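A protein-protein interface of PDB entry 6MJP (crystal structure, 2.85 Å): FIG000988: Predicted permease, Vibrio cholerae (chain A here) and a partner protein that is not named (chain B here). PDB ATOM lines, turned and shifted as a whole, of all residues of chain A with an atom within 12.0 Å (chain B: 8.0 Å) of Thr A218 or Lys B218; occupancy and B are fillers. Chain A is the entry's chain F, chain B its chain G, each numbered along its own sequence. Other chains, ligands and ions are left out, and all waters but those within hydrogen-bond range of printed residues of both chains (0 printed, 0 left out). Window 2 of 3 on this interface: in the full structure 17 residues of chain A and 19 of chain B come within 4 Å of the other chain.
Printed residues of chain B within 4 Å of Pro A217: Asn B173, Val B186 and Thr B208.
Of the printed residues of chain B, Thr A218 touches Phe B188 (3.7 Å) and Lys B218 (3.1 Å).
Printed residues of chain B within 4 Å of Val A220: Ile B216 (3.7 Å) and Lys B218 (3.6 Å).
Asp A221 touches none of the printed residues of chain B.
No residue of chain A comes within 4 Å of Val B206.
No residue of chain A comes within 4 Å of Leu B207.
Thr B208 touches one residue of chain A.
Arg B209 touches none of the printed residues of chain A.
Printed residues of chain A within 4 Å of Ile B216: Val A220.
No residue of chain A comes within 4 Å of Ser B217.
Lys B218 touches two residues of chain A.
No residue of chain A comes within 4 Å of Glu B219.
No residue of chain A comes within 4 Å of Ser B220.
O of Thr A218 lies within hydrogen-bond range of NZ of Lys B218 (3.1 Å).
Among the printed residues, merely in contact across the chains: Pro A217 with Asn B173, Pro A217 with Thr B208, Val A220 with Lys B218, Thr A218 with Phe B188, Val A220 with Ile B216 and Pro A217 with Val B186.
Printed residues of chain B that touch a printed residue of chain A: Asn B173, Val B186, Phe B188, Thr B208, Ile B216 and Lys B218.
Hydrophobic or aromatic side chains of chain A that line the printed part of chain B: Pro A217 and Val A220.
Among the printed residues, 7 pairs touch across the chains.
Among the printed residues, no Asp or Glu carboxylate lies within 4 Å of a Lys or Arg side-chain nitrogen of the other chain.
The backbone carbonyl oxygen (O) of Phe B188 lies within hydrogen-bond range of the backbone NH (N) of Val B206 (2.9 Å).
O of Val B186 lies within hydrogen-bond range of N of Thr B208 (2.8 Å).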
ATOM      1  N   GLN A 176       9.668   6.710 -29.058  1.00  0.00           N
ATOM      2  CA  GLN A 176      10.550   5.610 -29.450  1.00  0.00           C
ATOM      3  C   GLN A 176       9.732   4.326 -29.368  1.00  0.00           C
ATOM      4  O   GLN A 176       9.564   3.753 -28.289  1.00  0.00           O
ATOM      5  CB  GLN A 176      11.789   5.547 -28.568  1.00  0.00           C
ATOM      6  CG  GLN A 176      12.662   4.328 -28.804  1.00  0.00           C
ATOM      7  CD  GLN A 176      13.805   4.226 -27.814  1.00  0.00           C
ATOM      8  OE1 GLN A 176      14.305   5.239 -27.322  1.00  0.00           O
ATOM      9  NE2 GLN A 176      14.221   3.000 -27.513  1.00  0.00           N
ATOM     10  N   LEU A 177       9.218   3.886 -30.511  1.00  0.00           N
ATOM     11  CA  LEU A 177       8.339   2.731 -30.577  1.00  0.00           C
ATOM     12  C   LEU A 177       9.086   1.437 -30.850  1.00  0.00           C
ATOM     13  O   LEU A 177       8.455   0.377 -30.928  1.00  0.00           O
ATOM     14  CB  LEU A 177       7.270   2.951 -31.652  1.00  0.00           C
ATOM     15  CG  LEU A 177       6.223   4.029 -31.358  1.00  0.00           C
ATOM     16  CD1 LEU A 177       5.405   4.296 -32.610  1.00  0.00           C
ATOM     17  CD2 LEU A 177       5.318   3.649 -30.178  1.00  0.00           C
ATOM     18  N   LEU A 184      13.575  -0.847 -23.398  1.00  0.00           N
ATOM     19  CA  LEU A 184      12.197  -0.996 -23.831  1.00  0.00           C
ATOM     20  C   LEU A 184      11.718   0.269 -24.528  1.00  0.00           C
ATOM     21  O   LEU A 184      12.265   1.355 -24.312  1.00  0.00           O
ATOM     22  CB  LEU A 184      11.307  -1.310 -22.627  1.00  0.00           C
ATOM     23  CG  LEU A 184      11.752  -2.516 -21.804  1.00  0.00           C
ATOM     24  CD1 LEU A 184      10.853  -2.702 -20.595  1.00  0.00           C
ATOM     25  CD2 LEU A 184      11.750  -3.756 -22.673  1.00  0.00           C
ATOM     26  N   PRO A 185      10.691   0.161 -25.379  1.00  0.00           N
ATOM     27  CA  PRO A 185      10.128   1.364 -26.006  1.00  0.00           C
ATOM     28  C   PRO A 185       9.632   2.355 -24.967  1.00  0.00           C
ATOM     29  O   PRO A 185       9.256   1.992 -23.850  1.00  0.00           O
ATOM     30  CB  PRO A 185       8.971   0.820 -26.853  1.00  0.00           C
ATOM     31  CG  PRO A 185       8.672  -0.534 -26.275  1.00  0.00           C
ATOM     32  CD  PRO A 185       9.993  -1.059 -25.813  1.00  0.00           C
ATOM     33  N   SER A 186       9.630   3.625 -25.346  1.00  0.00           N
ATOM     34  CA  SER A 186       9.295   4.664 -24.394  1.00  0.00           C
ATOM     35  C   SER A 186       8.733   5.859 -25.142  1.00  0.00           C
ATOM     36  O   SER A 186       8.846   5.963 -26.365  1.00  0.00           O
ATOM     37  CB  SER A 186      10.519   5.066 -23.568  1.00  0.00           C
ATOM     38  OG  SER A 186      11.577   5.464 -24.426  1.00  0.00           O
ATOM     39  N   VAL A 187       8.101   6.748 -24.379  1.00  0.00           N
ATOM     40  CA  VAL A 187       7.590   8.026 -24.857  1.00  0.00           C
ATOM     41  C   VAL A 187       7.783   9.009 -23.712  1.00  0.00           C
ATOM     42  O   VAL A 187       7.285   8.774 -22.604  1.00  0.00           O
ATOM     43  CB  VAL A 187       6.104   7.959 -25.266  1.00  0.00           C
ATOM     44  CG1 VAL A 187       5.521   9.357 -25.381  1.00  0.00           C
ATOM     45  CG2 VAL A 187       5.920   7.215 -26.574  1.00  0.00           C
ATOM     46  N   TYR A 213       7.784   7.879 -20.058  1.00  0.00           N
ATOM     47  CA  TYR A 213       6.866   6.753 -19.885  1.00  0.00           C
ATOM     48  C   TYR A 213       7.389   5.566 -20.687  1.00  0.00           C
ATOM     49  O   TYR A 213       7.306   5.564 -21.918  1.00  0.00           O
ATOM     50  CB  TYR A 213       5.446   7.130 -20.321  1.00  0.00           C
ATOM     51  CG  TYR A 213       4.922   8.406 -19.682  1.00  0.00           C
ATOM     52  CD1 TYR A 213       5.243   9.652 -20.203  1.00  0.00           C
ATOM     53  CD2 TYR A 213       4.107   8.363 -18.557  1.00  0.00           C
ATOM     54  CE1 TYR A 213       4.775  10.818 -19.619  1.00  0.00           C
ATOM     55  CE2 TYR A 213       3.636   9.524 -17.966  1.00  0.00           C
ATOM     56  CZ  TYR A 213       3.970  10.747 -18.500  1.00  0.00           C
ATOM     57  OH  TYR A 213       3.501  11.901 -17.915  1.00  0.00           O
ATOM     58  N   GLU A 214       7.928   4.556 -19.995  1.00  0.00           N
ATOM     59  CA  GLU A 214       8.481   3.360 -20.632  1.00  0.00           C
ATOM     60  C   GLU A 214       7.436   2.249 -20.614  1.00  0.00           C
ATOM     61  O   GLU A 214       7.079   1.741 -19.545  1.00  0.00           O
ATOM     62  CB  GLU A 214       9.757   2.902 -19.927  1.00  0.00           C
ATOM     63  CG  GLU A 214      10.507   1.809 -20.678  1.00  0.00           C
ATOM     64  CD  GLU A 214      11.824   1.429 -20.028  1.00  0.00           C
ATOM     65  OE1 GLU A 214      11.856   1.281 -18.792  1.00  0.00           O
ATOM     66  OE2 GLU A 214      12.831   1.286 -20.758  1.00  0.00           O
ATOM     67  N   GLY A 215       6.961   1.854 -21.789  1.00  0.00           N
ATOM     68  CA  GLY A 215       5.944   0.826 -21.847  1.00  0.00           C
ATOM     69  C   GLY A 215       5.363   0.700 -23.240  1.00  0.00           C
ATOM     70  O   GLY A 215       5.892   1.245 -24.207  1.00  0.00           O
ATOM     71  N   VAL A 216       4.260  -0.039 -23.315  1.00  0.00           N
ATOM     72  CA  VAL A 216       3.577  -0.334 -24.573  1.00  0.00           C
ATOM     73  C   VAL A 216       2.092  -0.022 -24.399  1.00  0.00           C
ATOM     74  O   VAL A 216       1.534  -0.265 -23.316  1.00  0.00           O
ATOM     75  CB  VAL A 216       3.817  -1.793 -24.996  1.00  0.00           C
ATOM     76  CG1 VAL A 216       2.931  -2.188 -26.166  1.00  0.00           C
ATOM     77  CG2 VAL A 216       5.278  -2.001 -25.359  1.00  0.00           C
ATOM     78  N   PRO A 217       1.424   0.535 -25.419  1.00  0.00           N
ATOM     79  CA  PRO A 217      -0.007   0.870 -25.272  1.00  0.00           C
ATOM     80  C   PRO A 217      -0.898  -0.298 -24.871  1.00  0.00           C
ATOM     81  O   PRO A 217      -1.931  -0.075 -24.221  1.00  0.00           O
ATOM     82  CB  PRO A 217      -0.374   1.401 -26.665  1.00  0.00           C
ATOM     83  CG  PRO A 217       0.897   1.973 -27.180  1.00  0.00           C
ATOM     84  CD  PRO A 217       1.996   1.094 -26.656  1.00  0.00           C
ATOM     85  N   THR A 218      -0.543  -1.528 -25.248  1.00  0.00           N
ATOM     86  CA  THR A 218      -1.350  -2.697 -24.924  1.00  0.00           C
ATOM     87  C   THR A 218      -1.089  -3.226 -23.513  1.00  0.00           C
ATOM     88  O   THR A 218      -2.031  -3.640 -22.827  1.00  0.00           O
ATOM     89  CB  THR A 218      -1.108  -3.793 -25.963  1.00  0.00           C
ATOM     90  OG1 THR A 218       0.298  -4.002 -26.121  1.00  0.00           O
ATOM     91  CG2 THR A 218      -1.688  -3.381 -27.300  1.00  0.00           C
ATOM     92  N   ARG A 219       0.162  -3.221 -23.053  1.00  0.00           N
ATOM     93  CA  ARG A 219       0.463  -3.648 -21.693  1.00  0.00           C
ATOM     94  C   ARG A 219       0.279  -2.492 -20.704  1.00  0.00           C
ATOM     95  O   ARG A 219       0.080  -1.335 -21.085  1.00  0.00           O
ATOM     96  CB  ARG A 219       1.885  -4.204 -21.600  1.00  0.00           C
ATOM     97  CG  ARG A 219       1.974  -5.722 -21.653  1.00  0.00           C
ATOM     98  CD  ARG A 219       3.360  -6.204 -21.248  1.00  0.00           C
ATOM     99  NE  ARG A 219       3.356  -7.608 -20.851  1.00  0.00           N
ATOM    100  CZ  ARG A 219       4.406  -8.244 -20.338  1.00  0.00           C
ATOM    101  NH1 ARG A 219       5.551  -7.599 -20.157  1.00  0.00           N
ATOM    102  NH2 ARG A 219       4.311  -9.524 -20.002  1.00  0.00           N
ATOM    103  N   VAL A 220       0.363  -2.820 -19.413  1.00  0.00           N
ATOM    104  CA  VAL A 220       0.095  -1.855 -18.352  1.00  0.00           C
ATOM    105  C   VAL A 220       1.282  -1.629 -17.415  1.00  0.00           C
ATOM    106  O   VAL A 220       1.336  -0.584 -16.749  1.00  0.00           O
ATOM    107  CB  VAL A 220      -1.150  -2.265 -17.534  1.00  0.00           C
ATOM    108  CG1 VAL A 220      -1.662  -1.099 -16.712  1.00  0.00           C
ATOM    109  CG2 VAL A 220      -2.248  -2.776 -18.446  1.00  0.00           C
ATOM    110  N   ASP A 221       2.238  -2.551 -17.320  1.00  0.00           N
ATOM    111  CA  ASP A 221       3.429  -2.340 -16.497  1.00  0.00           C
ATOM    112  C   ASP A 221       4.300  -1.265 -17.132  1.00  0.00           C
ATOM    113  O   ASP A 221       5.004  -1.523 -18.111  1.00  0.00           O
ATOM    114  CB  ASP A 221       4.200  -3.646 -16.338  1.00  0.00           C
ATOM    115  CG  ASP A 221       4.341  -4.413 -17.643  1.00  0.00           C
ATOM    116  OD1 ASP A 221       3.369  -4.449 -18.426  1.00  0.00           O
ATOM    117  OD2 ASP A 221       5.429  -4.979 -17.885  1.00  0.00           O
ATOM    118  N   TYR A 222       4.257  -0.047 -16.593  1.00  0.00           N
ATOM    119  CA  TYR A 222       5.078   1.052 -17.089  1.00  0.00           C
ATOM    120  C   TYR A 222       6.236   1.317 -16.134  1.00  0.00           C
ATOM    121  O   TYR A 222       6.334   0.735 -15.052  1.00  0.00           O
ATOM    122  CB  TYR A 222       4.254   2.338 -17.276  1.00  0.00           C
ATOM    123  CG  TYR A 222       3.313   2.353 -18.476  1.00  0.00           C
ATOM    124  CD1 TYR A 222       3.777   2.642 -19.754  1.00  0.00           C
ATOM    125  CD2 TYR A 222       1.956   2.103 -18.316  1.00  0.00           C
ATOM    126  CE1 TYR A 222       2.911   2.658 -20.844  1.00  0.00           C
ATOM    127  CE2 TYR A 222       1.091   2.120 -19.394  1.00  0.00           C
ATOM    128  CZ  TYR A 222       1.567   2.396 -20.653  1.00  0.00           C
ATOM    129  OH  TYR A 222       0.680   2.401 -21.710  1.00  0.00           O
ATOM    130  N   LEU B 172      -3.861   1.674 -34.692  1.00  0.00           N
ATOM    131  CA  LEU B 172      -3.812   3.038 -34.182  1.00  0.00           C
ATOM    132  C   LEU B 172      -3.265   3.074 -32.759  1.00  0.00           C
ATOM    133  O   LEU B 172      -3.651   2.265 -31.910  1.00  0.00           O
ATOM    134  CB  LEU B 172      -5.209   3.665 -34.210  1.00  0.00           C
ATOM    135  CG  LEU B 172      -5.258   5.198 -34.092  1.00  0.00           C
ATOM    136  CD1 LEU B 172      -6.459   5.778 -34.821  1.00  0.00           C
ATOM    137  CD2 LEU B 172      -5.256   5.660 -32.641  1.00  0.00           C
ATOM    138  N   ASN B 173      -2.374   4.031 -32.498  1.00  0.00           N
ATOM    139  CA  ASN B 173      -1.932   4.347 -31.144  1.00  0.00           C
ATOM    140  C   ASN B 173      -2.156   5.833 -30.911  1.00  0.00           C
ATOM    141  O   ASN B 173      -1.981   6.636 -31.830  1.00  0.00           O
ATOM    142  CB  ASN B 173      -0.450   3.995 -30.924  1.00  0.00           C
ATOM    143  CG  ASN B 173      -0.139   2.531 -31.207  1.00  0.00           C
ATOM    144  OD1 ASN B 173       0.073   1.740 -30.289  1.00  0.00           O
ATOM    145  ND2 ASN B 173      -0.089   2.170 -32.487  1.00  0.00           N
ATOM    146  N   VAL B 186      -4.104   6.580 -23.011  1.00  0.00           N
ATOM    147  CA  VAL B 186      -3.472   5.974 -24.180  1.00  0.00           C
ATOM    148  C   VAL B 186      -4.464   4.998 -24.796  1.00  0.00           C
ATOM    149  O   VAL B 186      -5.024   4.148 -24.092  1.00  0.00           O
ATOM    150  CB  VAL B 186      -2.159   5.244 -23.826  1.00  0.00           C
ATOM    151  CG1 VAL B 186      -1.568   4.601 -25.080  1.00  0.00           C
ATOM    152  CG2 VAL B 186      -1.144   6.175 -23.169  1.00  0.00           C
ATOM    153  N   ILE B 187      -4.659   5.094 -26.107  1.00  0.00           N
ATOM    154  CA  ILE B 187      -5.597   4.240 -26.827  1.00  0.00           C
ATOM    155  C   ILE B 187      -4.849   3.461 -27.900  1.00  0.00           C
ATOM    156  O   ILE B 187      -3.941   3.993 -28.550  1.00  0.00           O
ATOM    157  CB  ILE B 187      -6.742   5.059 -27.459  1.00  0.00           C
ATOM    158  CG1 ILE B 187      -7.343   6.017 -26.423  1.00  0.00           C
ATOM    159  CG2 ILE B 187      -7.802   4.124 -28.057  1.00  0.00           C
ATOM    160  CD1 ILE B 187      -8.489   6.873 -26.935  1.00  0.00           C
ATOM    161  N   PHE B 188      -5.237   2.199 -28.086  1.00  0.00           N
ATOM    162  CA  PHE B 188      -4.738   1.358 -29.164  1.00  0.00           C
ATOM    163  C   PHE B 188      -5.908   0.621 -29.802  1.00  0.00           C
ATOM    164  O   PHE B 188      -6.855   0.225 -29.118  1.00  0.00           O
ATOM    165  CB  PHE B 188      -3.696   0.350 -28.658  1.00  0.00           C
ATOM    166  CG  PHE B 188      -3.216  -0.598 -29.711  1.00  0.00           C
ATOM    167  CD1 PHE B 188      -2.180  -0.239 -30.548  1.00  0.00           C
ATOM    168  CD2 PHE B 188      -3.800  -1.850 -29.869  1.00  0.00           C
ATOM    169  CE1 PHE B 188      -1.731  -1.102 -31.526  1.00  0.00           C
ATOM    170  CE2 PHE B 188      -3.353  -2.714 -30.847  1.00  0.00           C
ATOM    171  CZ  PHE B 188      -2.317  -2.340 -31.676  1.00  0.00           C
ATOM    172  N   SER B 189      -5.841   0.426 -31.117  1.00  0.00           N
ATOM    173  CA  SER B 189      -6.910  -0.282 -31.814  1.00  0.00           C
ATOM    174  C   SER B 189      -6.345  -1.067 -32.993  1.00  0.00           C
ATOM    175  O   SER B 189      -5.452  -0.591 -33.697  1.00  0.00           O
ATOM    176  CB  SER B 189      -7.998   0.690 -32.289  1.00  0.00           C
ATOM    177  OG  SER B 189      -9.031   0.026 -32.996  1.00  0.00           O
ATOM    178  N   GLU B 190      -6.867  -2.285 -33.190  1.00  0.00           N
ATOM    179  CA  GLU B 190      -6.472  -3.088 -34.344  1.00  0.00           C
ATOM    180  C   GLU B 190      -6.876  -2.412 -35.648  1.00  0.00           C
ATOM    181  O   GLU B 190      -6.069  -2.303 -36.579  1.00  0.00           O
ATOM    182  CB  GLU B 190      -7.084  -4.486 -34.261  1.00  0.00           C
ATOM    183  CG  GLU B 190      -6.336  -5.454 -33.354  1.00  0.00           C
ATOM    184  CD  GLU B 190      -6.788  -6.897 -33.529  1.00  0.00           C
ATOM    185  OE1 GLU B 190      -7.402  -7.216 -34.571  1.00  0.00           O
ATOM    186  OE2 GLU B 190      -6.523  -7.712 -32.621  1.00  0.00           O
ATOM    187  N   ALA B 205     -10.833  -1.862 -29.159  1.00  0.00           N
ATOM    188  CA  ALA B 205      -9.838  -0.902 -28.704  1.00  0.00           C
ATOM    189  C   ALA B 205      -9.569  -1.061 -27.215  1.00  0.00           C
ATOM    190  O   ALA B 205     -10.496  -1.252 -26.419  1.00  0.00           O
ATOM    191  CB  ALA B 205     -10.293   0.528 -28.988  1.00  0.00           C
ATOM    192  N   VAL B 206      -8.293  -0.968 -26.845  1.00  0.00           N
ATOM    193  CA  VAL B 206      -7.859  -1.031 -25.451  1.00  0.00           C
ATOM    194  C   VAL B 206      -7.456   0.371 -25.011  1.00  0.00           C
ATOM    195  O   VAL B 206      -6.599   1.014 -25.635  1.00  0.00           O
ATOM    196  CB  VAL B 206      -6.712  -2.040 -25.255  1.00  0.00           C
ATOM    197  CG1 VAL B 206      -5.617  -1.851 -26.299  1.00  0.00           C
ATOM    198  CG2 VAL B 206      -6.142  -1.929 -23.848  1.00  0.00           C
ATOM    199  N   LEU B 207      -8.072   0.846 -23.930  1.00  0.00           N
ATOM    200  CA  LEU B 207      -7.909   2.216 -23.453  1.00  0.00           C
ATOM    201  C   LEU B 207      -7.304   2.207 -22.057  1.00  0.00           C
ATOM    202  O   LEU B 207      -7.845   1.568 -21.153  1.00  0.00           O
ATOM    203  CB  LEU B 207      -9.255   2.950 -23.418  1.00  0.00           C
ATOM    204  CG  LEU B 207      -9.336   4.132 -22.446  1.00  0.00           C
ATOM    205  CD1 LEU B 207      -8.386   5.242 -22.852  1.00  0.00           C
ATOM    206  CD2 LEU B 207     -10.753   4.639 -22.422  1.00  0.00           C
ATOM    207  N   THR B 208      -6.220   2.949 -21.868  1.00  0.00           N
ATOM    208  CA  THR B 208      -5.485   2.982 -20.611  1.00  0.00           C
ATOM    209  C   THR B 208      -5.574   4.366 -20.010  1.00  0.00           C
ATOM    210  O   THR B 208      -5.245   5.342 -20.680  1.00  0.00           O
ATOM    211  CB  THR B 208      -4.017   2.621 -20.829  1.00  0.00           C
ATOM    212  OG1 THR B 208      -3.916   1.581 -21.810  1.00  0.00           O
ATOM    213  CG2 THR B 208      -3.420   2.128 -19.550  1.00  0.00           C
ATOM    214  N   ARG B 209      -6.004   4.465 -18.753  1.00  0.00           N
ATOM    215  CA  ARG B 209      -6.043   5.759 -18.078  1.00  0.00           C
ATOM    216  C   ARG B 209      -5.155   5.733 -16.841  1.00  0.00           C
ATOM    217  O   ARG B 209      -5.001   4.694 -16.191  1.00  0.00           O
ATOM    218  CB  ARG B 209      -7.475   6.157 -17.671  1.00  0.00           C
ATOM    219  CG  ARG B 209      -8.396   6.421 -18.847  1.00  0.00           C
ATOM    220  CD  ARG B 209      -9.768   6.876 -18.377  1.00  0.00           C
ATOM    221  N   LEU B 210      -4.574   6.884 -16.518  1.00  0.00           N
ATOM    222  CA  LEU B 210      -3.660   7.015 -15.389  1.00  0.00           C
ATOM    223  C   LEU B 210      -4.284   7.895 -14.310  1.00  0.00           C
ATOM    224  O   LEU B 210      -4.789   8.982 -14.613  1.00  0.00           O
ATOM    225  CB  LEU B 210      -2.320   7.611 -15.837  1.00  0.00           C
ATOM    226  CG  LEU B 210      -1.370   6.771 -16.697  1.00  0.00           C
ATOM    227  CD1 LEU B 210      -1.933   6.466 -18.085  1.00  0.00           C
ATOM    228  CD2 LEU B 210      -0.028   7.469 -16.818  1.00  0.00           C
ATOM    229  N   GLU B 215      -2.509   4.200  -9.668  1.00  0.00           N
ATOM    230  CA  GLU B 215      -3.530   3.416 -10.355  1.00  0.00           C
ATOM    231  C   GLU B 215      -3.454   3.663 -11.856  1.00  0.00           C
ATOM    232  O   GLU B 215      -3.420   4.816 -12.307  1.00  0.00           O
ATOM    233  CB  GLU B 215      -4.936   3.752  -9.838  1.00  0.00           C
ATOM    234  N   ILE B 216      -3.425   2.569 -12.619  1.00  0.00           N
ATOM    235  CA  ILE B 216      -3.470   2.579 -14.080  1.00  0.00           C
ATOM    236  C   ILE B 216      -4.453   1.496 -14.505  1.00  0.00           C
ATOM    237  O   ILE B 216      -4.232   0.312 -14.217  1.00  0.00           O
ATOM    238  CB  ILE B 216      -2.089   2.322 -14.708  1.00  0.00           C
ATOM    239  CG1 ILE B 216      -1.048   3.273 -14.129  1.00  0.00           C
ATOM    240  CG2 ILE B 216      -2.142   2.517 -16.204  1.00  0.00           C
ATOM    241  CD1 ILE B 216       0.343   3.009 -14.633  1.00  0.00           C
ATOM    242  N   SER B 217      -5.543   1.890 -15.166  1.00  0.00           N
ATOM    243  CA  SER B 217      -6.644   0.985 -15.482  1.00  0.00           C
ATOM    244  C   SER B 217      -6.873   0.925 -16.979  1.00  0.00           C
ATOM    245  O   SER B 217      -7.122   1.956 -17.611  1.00  0.00           O
ATOM    246  CB  SER B 217      -7.940   1.429 -14.794  1.00  0.00           C
ATOM    247  OG  SER B 217      -8.987   0.499 -15.032  1.00  0.00           O
ATOM    248  N   LYS B 218      -6.821  -0.279 -17.544  1.00  0.00           N
ATOM    249  CA  LYS B 218      -7.084  -0.463 -18.968  1.00  0.00           C
ATOM    250  C   LYS B 218      -8.383  -1.239 -19.166  1.00  0.00           C
ATOM    251  O   LYS B 218      -8.756  -2.087 -18.348  1.00  0.00           O
ATOM    252  CB  LYS B 218      -5.930  -1.181 -19.672  1.00  0.00           C
ATOM    253  CG  LYS B 218      -5.971  -2.696 -19.606  1.00  0.00           C
ATOM    254  CD  LYS B 218      -5.043  -3.306 -20.646  1.00  0.00           C
ATOM    255  CE  LYS B 218      -5.072  -4.824 -20.574  1.00  0.00           C
ATOM    256  NZ  LYS B 218      -4.177  -5.446 -21.585  1.00  0.00           N
ATOM    257  N   GLU B 219      -9.069  -0.955 -20.262  1.00  0.00           N
ATOM    258  CA  GLU B 219     -10.360  -1.549 -20.538  1.00  0.00           C
ATOM    259  C   GLU B 219     -10.393  -1.974 -21.990  1.00  0.00           C
ATOM    260  O   GLU B 219     -10.041  -1.186 -22.873  1.00  0.00           O
ATOM    261  CB  GLU B 219     -11.486  -0.550 -20.231  1.00  0.00           C
ATOM    262  CG  GLU B 219     -12.870  -1.180 -20.196  1.00  0.00           C
ATOM    263  CD  GLU B 219     -13.958  -0.181 -19.861  1.00  0.00           C
ATOM    264  OE1 GLU B 219     -13.675   1.032 -19.987  1.00  0.00           O
ATOM    265  OE2 GLU B 219     -15.069  -0.599 -19.455  1.00  0.00           O
ATOM    266  N   SER B 220     -10.802  -3.221 -22.242  1.00  0.00           N
ATOM    267  CA  SER B 220     -10.836  -3.744 -23.605  1.00  0.00           C
ATOM    268  C   SER B 220     -12.249  -3.541 -24.141  1.00  0.00           C
ATOM    269  O   SER B 220     -13.115  -4.408 -24.057  1.00  0.00           O
ATOM    270  CB  SER B 220     -10.406  -5.198 -23.609  1.00  0.00           C
ATOM    271  OG  SER B 220     -10.408  -5.718 -24.929  1.00  0.00           O
ATOM    272  N   LEU B 221     -12.490  -2.332 -24.669  1.00  0.00           N
ATOM    273  CA  LEU B 221     -13.787  -1.943 -25.220  1.00  0.00           C
ATOM    274  C   LEU B 221     -14.014  -2.596 -26.584  1.00  0.00           C
ATOM    275  O   LEU B 221     -13.104  -2.614 -27.418  1.00  0.00           O
ATOM    276  CB  LEU B 221     -13.870  -0.423 -25.371  1.00  0.00           C
ATOM    277  CG  LEU B 221     -13.767   0.371 -24.070  1.00  0.00           C
ATOM    278  CD1 LEU B 221     -13.803   1.873 -24.334  1.00  0.00           C
ATOM    279  CD2 LEU B 221     -14.882  -0.054 -23.118  1.00  0.00           C
